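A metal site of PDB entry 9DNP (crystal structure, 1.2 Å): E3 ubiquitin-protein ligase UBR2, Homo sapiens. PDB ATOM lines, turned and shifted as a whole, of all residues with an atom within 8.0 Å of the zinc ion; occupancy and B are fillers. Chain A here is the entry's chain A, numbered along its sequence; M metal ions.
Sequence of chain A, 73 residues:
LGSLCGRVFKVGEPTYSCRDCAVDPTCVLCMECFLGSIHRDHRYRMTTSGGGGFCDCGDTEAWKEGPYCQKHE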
ATOM      1  N   SER A  17      25.516  20.773   4.391  1.00  0.00           N
ATOM      2  CA  SER A  17      24.842  19.639   5.000  1.00  0.00           C
ATOM      3  C   SER A  17      25.643  18.381   4.690  1.00  0.00           C
ATOM      4  O   SER A  17      25.714  17.956   3.528  1.00  0.00           O
ATOM      5  CB  SER A  17      23.417  19.503   4.483  1.00  0.00           C
ATOM      6  OG  SER A  17      22.728  18.485   5.197  1.00  0.00           O
ATOM      7  N   CYS A  18      26.245  17.783   5.711  1.00  0.00           N
ATOM      8  CA  CYS A  18      26.963  16.530   5.517  1.00  0.00           C
ATOM      9  C   CYS A  18      25.987  15.429   5.125  1.00  0.00           C
ATOM     10  O   CYS A  18      25.043  15.136   5.865  1.00  0.00           O
ATOM     11  CB  CYS A  18      27.682  16.133   6.792  1.00  0.00           C
ATOM     12  SG  CYS A  18      28.673  14.668   6.483  1.00  0.00           S
ATOM     13  N   ARG A  19      26.230  14.806   3.971  1.00  0.00           N
ATOM     14  CA  ARG A  19      25.340  13.730   3.547  1.00  0.00           C
ATOM     15  C   ARG A  19      25.490  12.492   4.419  1.00  0.00           C
ATOM     16  O   ARG A  19      24.547  11.716   4.565  1.00  0.00           O
ATOM     17  CB  ARG A  19      25.604  13.376   2.077  1.00  0.00           C
ATOM     18  CG  ARG A  19      25.309  14.520   1.125  1.00  0.00           C
ATOM     19  CD  ARG A  19      25.686  14.160  -0.300  1.00  0.00           C
ATOM     20  NE  ARG A  19      25.410  15.268  -1.217  1.00  0.00           N
ATOM     21  CZ  ARG A  19      24.248  15.467  -1.814  1.00  0.00           C
ATOM     22  NH1 ARG A  19      23.206  14.679  -1.598  1.00  0.00           N
ATOM     23  NH2 ARG A  19      24.121  16.487  -2.660  1.00  0.00           N
ATOM     24  N   ASP A  20      26.668  12.300   5.018  1.00  0.00           N
ATOM     25  CA  ASP A  20      26.930  11.117   5.822  1.00  0.00           C
ATOM     26  C   ASP A  20      26.397  11.247   7.237  1.00  0.00           C
ATOM     27  O   ASP A  20      26.075  10.225   7.875  1.00  0.00           O
ATOM     28  CB  ASP A  20      28.429  10.839   5.861  1.00  0.00           C
ATOM     29  CG  ASP A  20      29.000  10.499   4.497  1.00  0.00           C
ATOM     30  OD1 ASP A  20      28.372   9.690   3.786  1.00  0.00           O
ATOM     31  OD2 ASP A  20      30.062  11.049   4.148  1.00  0.00           O
ATOM     32  N   CYS A  21      26.275  12.461   7.756  1.00  0.00           N
ATOM     33  CA  CYS A  21      25.994  12.676   9.170  1.00  0.00           C
ATOM     34  C   CYS A  21      24.719  13.440   9.467  1.00  0.00           C
ATOM     35  O   CYS A  21      24.219  13.341  10.587  1.00  0.00           O
ATOM     36  CB  CYS A  21      27.180  13.369   9.860  1.00  0.00           C
ATOM     37  SG  CYS A  21      28.769  12.492   9.655  1.00  0.00           S
ATOM     38  N   ALA A  22      24.170  14.193   8.513  1.00  0.00           N
ATOM     39  CA  ALA A  22      22.958  14.958   8.785  1.00  0.00           C
ATOM     40  C   ALA A  22      21.805  14.028   9.131  1.00  0.00           C
ATOM     41  O   ALA A  22      21.570  13.027   8.455  1.00  0.00           O
ATOM     42  CB  ALA A  22      22.577  15.806   7.577  1.00  0.00           C
ATOM     43  N   LEU A  29      25.512  23.339   8.599  1.00  0.00           N
ATOM     44  CA  LEU A  29      26.548  24.095   9.284  1.00  0.00           C
ATOM     45  C   LEU A  29      26.885  25.324   8.459  1.00  0.00           C
ATOM     46  O   LEU A  29      26.852  25.294   7.217  1.00  0.00           O
ATOM     47  CB  LEU A  29      27.815  23.250   9.408  1.00  0.00           C
ATOM     48  CG  LEU A  29      27.639  22.004  10.265  1.00  0.00           C
ATOM     49  CD1 LEU A  29      28.914  21.163  10.192  1.00  0.00           C
ATOM     50  CD2 LEU A  29      27.296  22.355  11.697  1.00  0.00           C
ATOM     51  N   PHE A  34      31.543  24.337   9.335  1.00  0.00           N
ATOM     52  CA  PHE A  34      31.806  23.213   8.436  1.00  0.00           C
ATOM     53  C   PHE A  34      33.297  22.999   8.247  1.00  0.00           C
ATOM     54  O   PHE A  34      33.790  21.877   8.368  1.00  0.00           O
ATOM     55  CB  PHE A  34      31.128  23.453   7.089  1.00  0.00           C
ATOM     56  CG  PHE A  34      31.395  22.363   6.095  1.00  0.00           C
ATOM     57  CD1 PHE A  34      30.799  21.124   6.263  1.00  0.00           C
ATOM     58  CD2 PHE A  34      32.233  22.576   5.023  1.00  0.00           C
ATOM     59  CE1 PHE A  34      31.035  20.111   5.359  1.00  0.00           C
ATOM     60  CE2 PHE A  34      32.465  21.561   4.110  1.00  0.00           C
ATOM     61  CZ  PHE A  34      31.865  20.329   4.290  1.00  0.00           C
ATOM     62  N   SER A  37      35.106  21.330  11.117  1.00  0.00           N
ATOM     63  CA  SER A  37      34.478  20.099  11.585  1.00  0.00           C
ATOM     64  C   SER A  37      35.044  18.894  10.859  1.00  0.00           C
ATOM     65  O   SER A  37      35.730  19.013   9.842  1.00  0.00           O
ATOM     66  CB  SER A  37      32.964  20.146  11.375  1.00  0.00           C
ATOM     67  OG  SER A  37      32.627  19.942  10.012  1.00  0.00           O
ATOM     68  N   ILE A  38      34.726  17.706  11.377  1.00  0.00           N
ATOM     69  CA  ILE A  38      35.103  16.468  10.708  1.00  0.00           C
ATOM     70  C   ILE A  38      34.437  16.323   9.349  1.00  0.00           C
ATOM     71  O   ILE A  38      34.911  15.568   8.495  1.00  0.00           O
ATOM     72  CB  ILE A  38      34.797  15.233  11.589  1.00  0.00           C
ATOM     73  CG1 ILE A  38      33.279  15.068  11.751  1.00  0.00           C
ATOM     74  CG2 ILE A  38      35.515  15.328  12.934  1.00  0.00           C
ATOM     75  CD1 ILE A  38      32.850  13.716  12.309  1.00  0.00           C
ATOM     76  N   HIS A  39      33.341  17.054   9.115  1.00  0.00           N
ATOM     77  CA  HIS A  39      32.532  16.841   7.916  1.00  0.00           C
ATOM     78  C   HIS A  39      33.150  17.442   6.665  1.00  0.00           C
ATOM     79  O   HIS A  39      32.697  17.118   5.569  1.00  0.00           O
ATOM     80  CB  HIS A  39      31.109  17.380   8.125  1.00  0.00           C
ATOM     81  CG  HIS A  39      30.508  16.948   9.424  1.00  0.00           C
ATOM     82  ND1 HIS A  39      30.097  15.658   9.668  1.00  0.00           N
ATOM     83  CD2 HIS A  39      30.322  17.632  10.575  1.00  0.00           C
ATOM     84  CE1 HIS A  39      29.649  15.566  10.911  1.00  0.00           C
ATOM     85  NE2 HIS A  39      29.777  16.754  11.486  1.00  0.00           N
ATOM     86  N   ARG A  40      34.157  18.295   6.816  1.00  0.00           N
ATOM     87  CA  ARG A  40      34.859  18.829   5.655  1.00  0.00           C
ATOM     88  C   ARG A  40      35.466  17.724   4.805  1.00  0.00           C
ATOM     89  O   ARG A  40      35.721  17.933   3.614  1.00  0.00           O
ATOM     90  CB  ARG A  40      35.919  19.822   6.103  1.00  0.00           C
ATOM     91  CG  ARG A  40      37.120  19.193   6.758  1.00  0.00           C
ATOM     92  CD  ARG A  40      38.296  20.146   6.736  1.00  0.00           C
ATOM     93  NE  ARG A  40      38.650  20.474   5.359  1.00  0.00           N
ATOM     94  CZ  ARG A  40      38.660  21.701   4.839  1.00  0.00           C
ATOM     95  NH1 ARG A  40      38.399  22.762   5.588  1.00  0.00           N
ATOM     96  NH2 ARG A  40      38.958  21.860   3.555  1.00  0.00           N
ATOM     97  N   ASP A  41      35.702  16.546   5.386  1.00  0.00           N
ATOM     98  CA  ASP A  41      36.251  15.396   4.664  1.00  0.00           C
ATOM     99  C   ASP A  41      35.178  14.400   4.249  1.00  0.00           C
ATOM    100  O   ASP A  41      35.524  13.348   3.697  1.00  0.00           O
ATOM    101  CB  ASP A  41      37.298  14.689   5.524  1.00  0.00           C
ATOM    102  CG  ASP A  41      38.498  15.558   5.799  1.00  0.00           C
ATOM    103  OD1 ASP A  41      38.948  16.268   4.884  1.00  0.00           O
ATOM    104  OD2 ASP A  41      38.987  15.534   6.952  1.00  0.00           O
ATOM    105  N   HIS A  42      33.903  14.688   4.508  1.00  0.00           N
ATOM    106  CA  HIS A  42      32.789  13.812   4.186  1.00  0.00           C
ATOM    107  C   HIS A  42      32.094  14.288   2.922  1.00  0.00           C
ATOM    108  O   HIS A  42      32.404  15.332   2.344  1.00  0.00           O
ATOM    109  CB  HIS A  42      31.791  13.770   5.347  1.00  0.00           C
ATOM    110  CG  HIS A  42      32.345  13.209   6.621  1.00  0.00           C
ATOM    111  ND1 HIS A  42      31.653  13.252   7.820  1.00  0.00           N
ATOM    112  CD2 HIS A  42      33.523  12.581   6.885  1.00  0.00           C
ATOM    113  CE1 HIS A  42      32.381  12.676   8.763  1.00  0.00           C
ATOM    114  NE2 HIS A  42      33.518  12.275   8.224  1.00  0.00           N
ATOM    115  N   ARG A  43      31.134  13.479   2.470  1.00  0.00           N
ATOM    116  CA  ARG A  43      30.274  13.909   1.372  1.00  0.00           C
ATOM    117  C   ARG A  43      29.298  14.953   1.904  1.00  0.00           C
ATOM    118  O   ARG A  43      28.715  14.787   2.971  1.00  0.00           O
ATOM    119  CB  ARG A  43      29.482  12.726   0.828  1.00  0.00           C
ATOM    120  CG  ARG A  43      30.328  11.596   0.241  1.00  0.00           C
ATOM    121  CD  ARG A  43      29.521  10.309   0.163  1.00  0.00           C
ATOM    122  NE  ARG A  43      28.135  10.572  -0.207  1.00  0.00           N
ATOM    123  CZ  ARG A  43      27.075  10.112   0.446  1.00  0.00           C
ATOM    124  NH1 ARG A  43      27.204   9.408   1.553  1.00  0.00           N
ATOM    125  NH2 ARG A  43      25.860  10.367  -0.031  1.00  0.00           N
ATOM    126  N   TYR A  44      29.109  16.038   1.146  1.00  0.00           N
ATOM    127  CA  TYR A  44      28.310  17.142   1.643  1.00  0.00           C
ATOM    128  C   TYR A  44      27.534  17.816   0.508  1.00  0.00           C
ATOM    129  O   TYR A  44      27.849  17.669  -0.672  1.00  0.00           O
ATOM    130  CB  TYR A  44      29.181  18.179   2.374  1.00  0.00           C
ATOM    131  CG  TYR A  44      30.136  18.931   1.481  1.00  0.00           C
ATOM    132  CD1 TYR A  44      29.755  20.108   0.841  1.00  0.00           C
ATOM    133  CD2 TYR A  44      31.426  18.460   1.267  1.00  0.00           C
ATOM    134  CE1 TYR A  44      30.631  20.796   0.023  1.00  0.00           C
ATOM    135  CE2 TYR A  44      32.311  19.144   0.446  1.00  0.00           C
ATOM    136  CZ  TYR A  44      31.904  20.305  -0.175  1.00  0.00           C
ATOM    137  OH  TYR A  44      32.773  20.998  -0.990  1.00  0.00           O
ATOM    138  N   TRP A  63      22.894  15.714  14.165  1.00  0.00           N
ATOM    139  CA  TRP A  63      24.066  15.057  13.586  1.00  0.00           C
ATOM    140  C   TRP A  63      24.218  13.654  14.150  1.00  0.00           C
ATOM    141  O   TRP A  63      24.126  13.457  15.364  1.00  0.00           O
ATOM    142  CB  TRP A  63      25.349  15.875  13.864  1.00  0.00           C
ATOM    143  CG  TRP A  63      25.187  17.289  13.410  1.00  0.00           C
ATOM    144  CD1 TRP A  63      25.013  18.394  14.192  1.00  0.00           C
ATOM    145  CD2 TRP A  63      25.130  17.738  12.053  1.00  0.00           C
ATOM    146  NE1 TRP A  63      24.843  19.515  13.402  1.00  0.00           N
ATOM    147  CE2 TRP A  63      24.912  19.132  12.087  1.00  0.00           C
ATOM    148  CE3 TRP A  63      25.247  17.097  10.821  1.00  0.00           C
ATOM    149  CZ2 TRP A  63      24.822  19.901  10.927  1.00  0.00           C
ATOM    150  CZ3 TRP A  63      25.143  17.854   9.673  1.00  0.00           C
ATOM    151  CH2 TRP A  63      24.920  19.241   9.736  1.00  0.00           C
ATOM    152  N   LYS A  64      24.489  12.694  13.258  1.00  0.00           N
ATOM    153  CA  LYS A  64      24.737  11.320  13.687  1.00  0.00           C
ATOM    154  C   LYS A  64      26.120  11.173  14.311  1.00  0.00           C
ATOM    155  O   LYS A  64      26.338  10.271  15.129  1.00  0.00           O
ATOM    156  CB  LYS A  64      24.616  10.368  12.505  1.00  0.00           C
ATOM    157  CG  LYS A  64      23.266  10.409  11.811  1.00  0.00           C
ATOM    158  CD  LYS A  64      23.117   9.288  10.789  1.00  0.00           C
ATOM    159  CE  LYS A  64      22.184   9.717   9.661  1.00  0.00           C
ATOM    160  NZ  LYS A  64      22.456   8.991   8.391  1.00  0.00           N
ATOM    161  N   GLU A  65      27.066  12.018  13.929  1.00  0.00           N
ATOM    162  CA  GLU A  65      28.354  12.102  14.598  1.00  0.00           C
ATOM    163  C   GLU A  65      28.971  13.473  14.331  1.00  0.00           C
ATOM    164  O   GLU A  65      28.516  14.215  13.446  1.00  0.00           O
ATOM    165  CB  GLU A  65      29.305  10.966  14.191  1.00  0.00           C
ATOM    166  CG  GLU A  65      29.657  10.936  12.730  1.00  0.00           C
ATOM    167  CD  GLU A  65      30.864  10.062  12.445  1.00  0.00           C
ATOM    168  OE1 GLU A  65      31.152   9.813  11.251  1.00  0.00           O
ATOM    169  OE2 GLU A  65      31.533   9.631  13.402  1.00  0.00           O
ATOM    170  N   GLY A  66      29.992  13.803  15.115  1.00  0.00           N
ATOM    171  CA  GLY A  66      30.650  15.090  15.063  1.00  0.00           C
ATOM    172  C   GLY A  66      29.731  16.290  15.101  1.00  0.00           C
ATOM    173  O   GLY A  66      29.739  17.123  14.187  1.00  0.00           O
HETATM  174 ZN    ZN M   1      29.848  14.060   8.369  1.00  0.00          ZN
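The backbone carbonyl oxygen (O) of Glu 65 lies close to a ring nitrogen (NE2) of His 39.
SG of Cys 18 lies close to N of Asp 20, 3.4 Å away.
The side-chain sulfur of Cys 18 lies close to the backbone carbonyl oxygen of Arg 43 (3.5 Å).
O of Cys 21 is in hydrogen-bond range of N of Lys 64, 2.8 Å away.
N of His 39 sits close to OG of Ser 37 (3.1 Å).
A ring nitrogen (NE2) of His 39 lies within hydrogen-bond range of the backbone carbonyl oxygen (O) of Gly 66, at 2.7 Å.
The zinc ion is bound by a ring nitrogen (ND1) of His 42 (2.1 Å), a ring nitrogen (ND1) of His 39 (2.1 Å), the side-chain sulfur (SG) of Cys 21 (2.3 Å) and the side-chain sulfur (SG) of Cys 18 (2.3 Å).
The zinc ion has four donor atoms within binding distance.
Four residues have an atom within 4 Å of the zinc ion: Cys 18, Cys 21, His 39 and His 42.
The nearest printed residue that does not touch the zinc ion is Asp 20 (4.3 Å).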
